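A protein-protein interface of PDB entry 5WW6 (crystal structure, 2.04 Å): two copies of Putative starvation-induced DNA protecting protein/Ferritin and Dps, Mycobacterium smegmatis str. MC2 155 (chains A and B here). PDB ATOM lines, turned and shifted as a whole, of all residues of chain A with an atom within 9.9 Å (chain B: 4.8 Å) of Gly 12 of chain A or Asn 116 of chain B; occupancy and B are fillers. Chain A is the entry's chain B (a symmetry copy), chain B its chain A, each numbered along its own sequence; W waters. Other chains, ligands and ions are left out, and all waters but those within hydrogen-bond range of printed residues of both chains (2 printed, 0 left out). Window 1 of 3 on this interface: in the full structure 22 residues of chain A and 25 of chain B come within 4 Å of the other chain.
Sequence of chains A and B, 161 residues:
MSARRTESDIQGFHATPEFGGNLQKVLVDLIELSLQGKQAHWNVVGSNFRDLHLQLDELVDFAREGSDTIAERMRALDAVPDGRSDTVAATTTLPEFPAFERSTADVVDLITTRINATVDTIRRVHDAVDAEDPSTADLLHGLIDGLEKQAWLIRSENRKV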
ATOM      1  N   ARG A   5     -21.267  26.470 -28.873  1.00  0.00           N
ATOM      2  CA  ARG A   5     -21.984  25.264 -28.461  1.00  0.00           C
ATOM      3  C   ARG A   5     -23.361  25.246 -29.120  1.00  0.00           C
ATOM      4  O   ARG A   5     -23.959  26.298 -29.351  1.00  0.00           O
ATOM      5  CB  ARG A   5     -22.091  25.197 -26.940  1.00  0.00           C
ATOM      6  CG  ARG A   5     -20.745  24.949 -26.274  1.00  0.00           C
ATOM      7  CD  ARG A   5     -20.794  25.185 -24.775  1.00  0.00           C
ATOM      8  NE  ARG A   5     -21.490  24.107 -24.078  1.00  0.00           N
ATOM      9  CZ  ARG A   5     -21.635  24.016 -22.757  1.00  0.00           C
ATOM     10  NH1 ARG A   5     -21.130  24.944 -21.944  1.00  0.00           N
ATOM     11  NH2 ARG A   5     -22.283  22.981 -22.247  1.00  0.00           N
ATOM     12  N   GLU A   7     -26.186  23.063 -28.366  1.00  0.00           N
ATOM     13  CA  GLU A   7     -27.355  22.658 -27.581  1.00  0.00           C
ATOM     14  C   GLU A   7     -28.210  23.878 -27.253  1.00  0.00           C
ATOM     15  O   GLU A   7     -27.683  24.959 -26.969  1.00  0.00           O
ATOM     16  CB  GLU A   7     -26.947  21.889 -26.321  1.00  0.00           C
ATOM     17  CG  GLU A   7     -25.777  22.502 -25.574  1.00  0.00           C
ATOM     18  CD  GLU A   7     -24.820  21.473 -25.018  1.00  0.00           C
ATOM     19  OE1 GLU A   7     -25.264  20.592 -24.250  1.00  0.00           O
ATOM     20  OE2 GLU A   7     -23.617  21.559 -25.343  1.00  0.00           O
ATOM     21  N   SER A   8     -29.527  23.696 -27.330  1.00  0.00           N
ATOM     22  CA  SER A   8     -30.490  24.788 -27.165  1.00  0.00           C
ATOM     23  C   SER A   8     -30.676  25.167 -25.699  1.00  0.00           C
ATOM     24  O   SER A   8     -30.798  26.350 -25.383  1.00  0.00           O
ATOM     25  CB  SER A   8     -31.833  24.440 -27.815  1.00  0.00           C
ATOM     26  OG  SER A   8     -32.399  23.283 -27.229  1.00  0.00           O
ATOM     27  N   ASP A   9     -30.708  24.174 -24.810  1.00  0.00           N
ATOM     28  CA  ASP A   9     -30.673  24.455 -23.374  1.00  0.00           C
ATOM     29  C   ASP A   9     -29.471  23.838 -22.674  1.00  0.00           C
ATOM     30  O   ASP A   9     -29.260  22.624 -22.699  1.00  0.00           O
ATOM     31  CB  ASP A   9     -32.002  24.144 -22.660  1.00  0.00           C
ATOM     32  CG  ASP A   9     -32.517  22.748 -22.933  1.00  0.00           C
ATOM     33  OD1 ASP A   9     -33.501  22.628 -23.694  1.00  0.00           O
ATOM     34  OD2 ASP A   9     -31.957  21.776 -22.381  1.00  0.00           O
ATOM     35  N   ILE A  10     -28.669  24.722 -22.090  1.00  0.00           N
ATOM     36  CA  ILE A  10     -27.521  24.372 -21.266  1.00  0.00           C
ATOM     37  C   ILE A  10     -27.970  24.568 -19.820  1.00  0.00           C
ATOM     38  O   ILE A  10     -28.484  25.639 -19.451  1.00  0.00           O
ATOM     39  CB  ILE A  10     -26.286  25.248 -21.628  1.00  0.00           C
ATOM     40  CG1 ILE A  10     -25.701  24.799 -22.971  1.00  0.00           C
ATOM     41  CG2 ILE A  10     -25.212  25.182 -20.549  1.00  0.00           C
ATOM     42  CD1 ILE A  10     -24.941  25.858 -23.750  1.00  0.00           C
ATOM     43  N   GLN A  11     -27.799  23.520 -19.019  1.00  0.00           N
ATOM     44  CA  GLN A  11     -28.218  23.531 -17.623  1.00  0.00           C
ATOM     45  C   GLN A  11     -27.152  24.229 -16.777  1.00  0.00           C
ATOM     46  O   GLN A  11     -25.960  24.171 -17.085  1.00  0.00           O
ATOM     47  CB  GLN A  11     -28.494  22.100 -17.136  1.00  0.00           C
ATOM     48  CG  GLN A  11     -29.882  21.902 -16.521  1.00  0.00           C
ATOM     49  CD  GLN A  11     -30.303  20.435 -16.392  1.00  0.00           C
ATOM     50  OE1 GLN A  11     -31.346  20.034 -16.908  1.00  0.00           O
ATOM     51  NE2 GLN A  11     -29.498  19.632 -15.697  1.00  0.00           N
ATOM     52  N   GLY A  12     -27.598  24.924 -15.738  1.00  0.00           N
ATOM     53  CA  GLY A  12     -26.698  25.590 -14.800  1.00  0.00           C
ATOM     54  C   GLY A  12     -26.273  24.657 -13.683  1.00  0.00           C
ATOM     55  O   GLY A  12     -26.690  23.489 -13.639  1.00  0.00           O
ATOM     56  N   PHE A  13     -25.435  25.174 -12.786  1.00  0.00           N
ATOM     57  CA  PHE A  13     -24.944  24.419 -11.635  1.00  0.00           C
ATOM     58  C   PHE A  13     -26.068  24.272 -10.610  1.00  0.00           C
ATOM     59  O   PHE A  13     -26.647  25.269 -10.180  1.00  0.00           O
ATOM     60  CB  PHE A  13     -23.728  25.136 -11.028  1.00  0.00           C
ATOM     61  CG  PHE A  13     -22.977  24.332  -9.996  1.00  0.00           C
ATOM     62  CD1 PHE A  13     -21.931  23.488 -10.375  1.00  0.00           C
ATOM     63  CD2 PHE A  13     -23.288  24.443  -8.638  1.00  0.00           C
ATOM     64  CE1 PHE A  13     -21.221  22.756  -9.422  1.00  0.00           C
ATOM     65  CE2 PHE A  13     -22.586  23.707  -7.682  1.00  0.00           C
ATOM     66  CZ  PHE A  13     -21.553  22.866  -8.075  1.00  0.00           C
ATOM     67  N   HIS A  14     -26.387  23.029 -10.251  1.00  0.00           N
ATOM     68  CA  HIS A  14     -27.392  22.736  -9.226  1.00  0.00           C
ATOM     69  C   HIS A  14     -26.675  22.356  -7.939  1.00  0.00           C
ATOM     70  O   HIS A  14     -25.803  21.487  -7.951  1.00  0.00           O
ATOM     71  CB  HIS A  14     -28.293  21.565  -9.644  1.00  0.00           C
ATOM     72  CG  HIS A  14     -29.114  21.822 -10.869  1.00  0.00           C
ATOM     73  ND1 HIS A  14     -28.609  21.686 -12.145  1.00  0.00           N
ATOM     74  CD2 HIS A  14     -30.416  22.167 -11.013  1.00  0.00           C
ATOM     75  CE1 HIS A  14     -29.559  21.964 -13.023  1.00  0.00           C
ATOM     76  NE2 HIS A  14     -30.665  22.259 -12.363  1.00  0.00           N
ATOM     77  N   ALA A  15     -27.038  23.002  -6.832  1.00  0.00           N
ATOM     78  CA  ALA A  15     -26.567  22.577  -5.511  1.00  0.00           C
ATOM     79  C   ALA A  15     -27.171  21.217  -5.157  1.00  0.00           C
ATOM     80  O   ALA A  15     -28.344  20.968  -5.455  1.00  0.00           O
ATOM     81  CB  ALA A  15     -26.953  23.594  -4.459  1.00  0.00           C
ATOM     82  N   THR A  16     -26.373  20.344  -4.536  1.00  0.00           N
ATOM     83  CA  THR A  16     -26.910  19.121  -3.922  1.00  0.00           C
ATOM     84  C   THR A  16     -27.809  19.527  -2.754  1.00  0.00           C
ATOM     85  O   THR A  16     -27.660  20.640  -2.229  1.00  0.00           O
ATOM     86  CB  THR A  16     -25.813  18.165  -3.394  1.00  0.00           C
ATOM     87  OG1 THR A  16     -25.087  18.792  -2.328  1.00  0.00           O
ATOM     88  CG2 THR A  16     -24.870  17.701  -4.515  1.00  0.00           C
ATOM     89  N   ARG A  73     -28.068  33.135  -2.658  1.00  0.00           N
ATOM     90  CA  ARG A  73     -27.120  32.149  -3.189  1.00  0.00           C
ATOM     91  C   ARG A  73     -27.767  30.757  -3.279  1.00  0.00           C
ATOM     92  O   ARG A  73     -27.570  30.038  -4.265  1.00  0.00           O
ATOM     93  CB  ARG A  73     -25.813  32.121  -2.365  1.00  0.00           C
ATOM     94  CG  ARG A  73     -24.722  31.196  -2.920  1.00  0.00           C
ATOM     95  CD  ARG A  73     -24.337  31.567  -4.343  1.00  0.00           C
ATOM     96  NE  ARG A  73     -23.315  30.694  -4.935  1.00  0.00           N
ATOM     97  CZ  ARG A  73     -23.126  30.550  -6.249  1.00  0.00           C
ATOM     98  NH1 ARG A  73     -23.891  31.211  -7.131  1.00  0.00           N
ATOM     99  NH2 ARG A  73     -22.175  29.738  -6.688  1.00  0.00           N
ATOM    100  N   ARG A  75     -31.022  30.234  -3.659  1.00  0.00           N
ATOM    101  CA  ARG A  75     -31.928  30.352  -4.809  1.00  0.00           C
ATOM    102  C   ARG A  75     -31.196  30.289  -6.155  1.00  0.00           C
ATOM    103  O   ARG A  75     -31.669  29.631  -7.090  1.00  0.00           O
ATOM    104  CB  ARG A  75     -32.786  31.622  -4.697  1.00  0.00           C
ATOM    105  CG  ARG A  75     -33.783  31.621  -3.538  1.00  0.00           C
ATOM    106  CD  ARG A  75     -34.799  30.484  -3.616  1.00  0.00           C
ATOM    107  NE  ARG A  75     -35.645  30.564  -4.800  1.00  0.00           N
ATOM    108  CZ  ARG A  75     -35.701  29.651  -5.764  1.00  0.00           C
ATOM    109  NH1 ARG A  75     -34.985  28.528  -5.700  1.00  0.00           N
ATOM    110  NH2 ARG A  75     -36.507  29.856  -6.795  1.00  0.00           N
ATOM    111  N   ALA A  76     -30.039  30.952  -6.239  1.00  0.00           N
ATOM    112  CA  ALA A  76     -29.213  30.929  -7.448  1.00  0.00           C
ATOM    113  C   ALA A  76     -28.854  29.488  -7.831  1.00  0.00           C
ATOM    114  O   ALA A  76     -28.863  29.126  -9.008  1.00  0.00           O
ATOM    115  CB  ALA A  76     -27.951  31.758  -7.253  1.00  0.00           C
ATOM    116  N   LEU A  77     -28.586  28.663  -6.820  1.00  0.00           N
ATOM    117  CA  LEU A  77     -28.232  27.271  -7.050  1.00  0.00           C
ATOM    118  C   LEU A  77     -29.436  26.321  -6.955  1.00  0.00           C
ATOM    119  O   LEU A  77     -29.272  25.105  -6.898  1.00  0.00           O
ATOM    120  CB  LEU A  77     -27.076  26.861  -6.120  1.00  0.00           C
ATOM    121  CG  LEU A  77     -25.732  27.592  -6.339  1.00  0.00           C
ATOM    122  CD1 LEU A  77     -24.648  27.024  -5.444  1.00  0.00           C
ATOM    123  CD2 LEU A  77     -25.255  27.557  -7.789  1.00  0.00           C
ATOM    124  N   ASP A  78     -30.634  26.902  -6.970  1.00  0.00           N
ATOM    125  CA  ASP A  78     -31.913  26.181  -6.887  1.00  0.00           C
ATOM    126  C   ASP A  78     -32.170  25.405  -5.593  1.00  0.00           C
ATOM    127  O   ASP A  78     -32.972  24.476  -5.571  1.00  0.00           O
ATOM    128  CB  ASP A  78     -32.205  25.345  -8.162  1.00  0.00           C
ATOM    129  CG  ASP A  78     -33.323  25.940  -9.014  1.00  0.00           C
ATOM    130  OD1 ASP A  78     -34.075  26.820  -8.525  1.00  0.00           O
ATOM    131  OD2 ASP A  78     -33.483  25.506 -10.173  1.00  0.00           O
ATOM    132  N   ASP A 133     -18.585  23.962  -3.935  1.00  0.00           N
ATOM    133  CA  ASP A 133     -18.651  25.237  -4.653  1.00  0.00           C
ATOM    134  C   ASP A 133     -17.755  26.308  -4.030  1.00  0.00           C
ATOM    135  O   ASP A 133     -18.196  27.009  -3.107  1.00  0.00           O
ATOM    136  CB  ASP A 133     -20.109  25.737  -4.738  1.00  0.00           C
ATOM    137  CG  ASP A 133     -20.271  26.906  -5.705  1.00  0.00           C
ATOM    138  OD1 ASP A 133     -20.012  26.727  -6.919  1.00  0.00           O
ATOM    139  OD2 ASP A 133     -20.665  27.995  -5.254  1.00  0.00           O
ATOM    140  N   THR B 112     -31.011  32.734 -20.097  1.00  0.00           N
ATOM    141  CA  THR B 112     -30.633  31.804 -19.012  1.00  0.00           C
ATOM    142  C   THR B 112     -29.606  30.779 -19.511  1.00  0.00           C
ATOM    143  O   THR B 112     -28.593  30.547 -18.855  1.00  0.00           O
ATOM    144  CB  THR B 112     -31.867  31.108 -18.381  1.00  0.00           C
ATOM    145  OG1 THR B 112     -32.734  32.107 -17.829  1.00  0.00           O
ATOM    146  CG2 THR B 112     -31.459  30.115 -17.256  1.00  0.00           C
ATOM    147  N   THR B 113     -29.867  30.204 -20.683  1.00  0.00           N
ATOM    148  CA  THR B 113     -28.946  29.255 -21.330  1.00  0.00           C
ATOM    149  C   THR B 113     -27.576  29.892 -21.592  1.00  0.00           C
ATOM    150  O   THR B 113     -26.541  29.268 -21.350  1.00  0.00           O
ATOM    151  CB  THR B 113     -29.573  28.696 -22.625  1.00  0.00           C
ATOM    152  OG1 THR B 113     -30.679  27.858 -22.266  1.00  0.00           O
ATOM    153  CG2 THR B 113     -28.576  27.869 -23.445  1.00  0.00           C
ATOM    154  N   ARG B 114     -27.576  31.146 -22.044  1.00  0.00           N
ATOM    155  CA  ARG B 114     -26.324  31.828 -22.348  1.00  0.00           C
ATOM    156  C   ARG B 114     -25.524  32.233 -21.106  1.00  0.00           C
ATOM    157  O   ARG B 114     -24.295  32.167 -21.122  1.00  0.00           O
ATOM    158  CB  ARG B 114     -26.553  32.967 -23.346  1.00  0.00           C
ATOM    159  CG  ARG B 114     -26.696  32.405 -24.760  1.00  0.00           C
ATOM    160  CD  ARG B 114     -27.912  32.979 -25.449  1.00  0.00           C
ATOM    161  NE  ARG B 114     -28.142  32.374 -26.761  1.00  0.00           N
ATOM    162  CZ  ARG B 114     -28.858  31.273 -26.965  1.00  0.00           C
ATOM    163  NH1 ARG B 114     -29.410  30.622 -25.942  1.00  0.00           N
ATOM    164  NH2 ARG B 114     -29.012  30.812 -28.194  1.00  0.00           N
ATOM    165  N   ILE B 115     -26.217  32.602 -20.028  1.00  0.00           N
ATOM    166  CA  ILE B 115     -25.564  32.820 -18.727  1.00  0.00           C
ATOM    167  C   ILE B 115     -24.951  31.493 -18.238  1.00  0.00           C
ATOM    168  O   ILE B 115     -23.768  31.456 -17.862  1.00  0.00           O
ATOM    169  CB  ILE B 115     -26.529  33.393 -17.655  1.00  0.00           C
ATOM    170  CG1 ILE B 115     -27.057  34.781 -18.068  1.00  0.00           C
ATOM    171  CG2 ILE B 115     -25.841  33.447 -16.282  1.00  0.00           C
ATOM    172  CD1 ILE B 115     -28.261  35.259 -17.269  1.00  0.00           C
ATOM    173  N   ASN B 116     -25.748  30.417 -18.275  1.00  0.00           N
ATOM    174  CA  ASN B 116     -25.283  29.073 -17.883  1.00  0.00           C
ATOM    175  C   ASN B 116     -24.005  28.689 -18.629  1.00  0.00           C
ATOM    176  O   ASN B 116     -23.060  28.201 -18.014  1.00  0.00           O
ATOM    177  CB  ASN B 116     -26.368  28.007 -18.106  1.00  0.00           C
ATOM    178  CG  ASN B 116     -27.562  28.159 -17.171  1.00  0.00           C
ATOM    179  OD1 ASN B 116     -27.551  28.959 -16.236  1.00  0.00           O
ATOM    180  ND2 ASN B 116     -28.608  27.384 -17.429  1.00  0.00           N
ATOM    181  N   ALA B 117     -23.987  28.937 -19.941  1.00  0.00           N
ATOM    182  CA  ALA B 117     -22.803  28.712 -20.788  1.00  0.00           C
ATOM    183  C   ALA B 117     -21.597  29.556 -20.359  1.00  0.00           C
ATOM    184  O   ALA B 117     -20.462  29.061 -20.311  1.00  0.00           O
ATOM    185  CB  ALA B 117     -23.139  28.981 -22.249  1.00  0.00           C
ATOM    186  N   THR B 118     -21.842  30.828 -20.057  1.00  0.00           N
ATOM    187  CA  THR B 118     -20.776  31.735 -19.606  1.00  0.00           C
ATOM    188  C   THR B 118     -20.173  31.242 -18.290  1.00  0.00           C
ATOM    189  O   THR B 118     -18.946  31.148 -18.162  1.00  0.00           O
ATOM    190  CB  THR B 118     -21.272  33.192 -19.491  1.00  0.00           C
ATOM    191  OG1 THR B 118     -21.908  33.562 -20.716  1.00  0.00           O
ATOM    192  CG2 THR B 118     -20.101  34.165 -19.224  1.00  0.00           C
ATOM    193  N   VAL B 119     -21.040  30.898 -17.341  1.00  0.00           N
ATOM    194  CA  VAL B 119     -20.629  30.365 -16.044  1.00  0.00           C
ATOM    195  C   VAL B 119     -19.864  29.038 -16.218  1.00  0.00           C
ATOM    196  O   VAL B 119     -18.853  28.828 -15.550  1.00  0.00           O
ATOM    197  CB  VAL B 119     -21.832  30.220 -15.073  1.00  0.00           C
ATOM    198  CG1 VAL B 119     -21.434  29.513 -13.777  1.00  0.00           C
ATOM    199  CG2 VAL B 119     -22.391  31.593 -14.724  1.00  0.00           C
ATOM    200  N   ASP B 120     -20.337  28.180 -17.129  1.00  0.00           N
ATOM    201  CA  ASP B 120     -19.671  26.906 -17.371  1.00  0.00           C
ATOM    202  C   ASP B 120     -18.208  27.115 -17.813  1.00  0.00           C
ATOM    203  O   ASP B 120     -17.334  26.424 -17.325  1.00  0.00           O
ATOM    204  CB  ASP B 120     -20.454  26.035 -18.363  1.00  0.00           C
ATOM    205  CG  ASP B 120     -19.897  24.619 -18.470  1.00  0.00           C
ATOM    206  OD1 ASP B 120     -19.667  23.964 -17.429  1.00  0.00           O
ATOM    207  OD2 ASP B 120     -19.688  24.157 -19.605  1.00  0.00           O
ATOM    208  N   ALA B 151     -28.973  34.783 -13.536  1.00  0.00           N
ATOM    209  CA  ALA B 151     -29.688  33.627 -14.088  1.00  0.00           C
ATOM    210  C   ALA B 151     -30.940  33.325 -13.267  1.00  0.00           C
ATOM    211  O   ALA B 151     -32.003  33.141 -13.838  1.00  0.00           O
ATOM    212  CB  ALA B 151     -28.783  32.401 -14.170  1.00  0.00           C
HETATM  213  O   HOH W   1     -31.414  28.686 -25.953  1.00  0.00           O
HETATM  214  O   HOH W   2     -19.637  27.375 -22.407  1.00  0.00           O
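No position is printed for both chains.
O of Thr 112 of chain B lies close to OD1 of Asn 116 of chain B (3.2 Å).
OE2 of Glu 7 of chain A lies within salt-bridge range of NE of Arg 5 of chain A (3.6 Å).
The backbone carbonyl oxygen of Gly 12 of chain A sits at hydrogen-bond distance from a ring nitrogen (ND1) of His 14 of chain A, at 3.0 Å.
Among the printed residues, pairs that only touch across the chains: Asp 9 of chain A with Thr 113 of chain B (3.6 Å), Ile 10 of chain A with Thr 113 of chain B (3.4 Å), Ile 10 of chain A with Ala 117 of chain B (3.9 Å) and Gln 11 of chain A with Asn 116 of chain B (3.5 Å).
Of the 17 printed residues of chain A, 6 touch a printed residue of chain B.
Hydrophobic or aromatic side chains of chain A within 4 Å of the printed part of chain B: Ile 10.
Among the printed residues, Asp or Glu carboxylates within 4 Å of a Lys or Arg side-chain nitrogen of the other chain: Arg 5 of chain A with Asp 120 of chain B (2.9 Å).
Of the printed residues of chain B, Arg 5 of chain A touches Asp 120 (2.9 Å).
Printed residues of chain B within 4 Å of Asp 9 of chain A: Thr 113.
Printed residues of chain B within 4 Å of Gln 11 of chain A: Asn 116.
Gly 12 of chain A touches one residue of chain B.
Thr 113 of chain B touches just these residues of chain A: Ser 8 (3.3 Å), Asp 9 (3.6 Å) and Ile 10 (3.4 Å).
Asn 116 of chain B touches just these residues of chain A: Ile 10 (2.7 Å), Gln 11 (3.5 Å) and Gly 12 (3.2 Å).
Thr 118 of chain B touches none of the printed residues of chain A.
Val 119 of chain B touches none of the printed residues of chain A.
The nearest printed residue of chain B that does not touch Gly 12 of chain A is Thr 112 of chain B (6.5 Å).
The nearest residue of chain A that does not touch Asn 116 of chain B is Arg 5 of chain A (5.5 Å).
Water W1 lies within hydrogen-bond range of O of Ser 8 of chain A (2.5 Å) and NH1 of Arg 114 of chain B (2.8 Å).
Water W2 bridges the backbone carbonyl oxygen (O) of Ala 117 of chain B (2.8 Å) and the guanidinium group (NH1) of Arg 5 of chain A (2.9 Å).
OG1 of Thr 113 of chain B lies close to O of Ser 8 of chain A (3.5 Å).
The side-chain amide nitrogen of Asn 116 of chain B lies within hydrogen-bond range of the backbone carbonyl oxygen of Ile 10 of chain A, at 2.7 Å.
The side-chain amide nitrogen of Asn 116 of chain B sits close to the backbone NH of Gly 12 of chain A, at 3.2 Å.
The side-chain carboxylate (OD2) of Asp 120 of chain B lies within salt-bridge range of the guanidinium group (NH1) of Arg 5 of chain A (2.9 Å).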
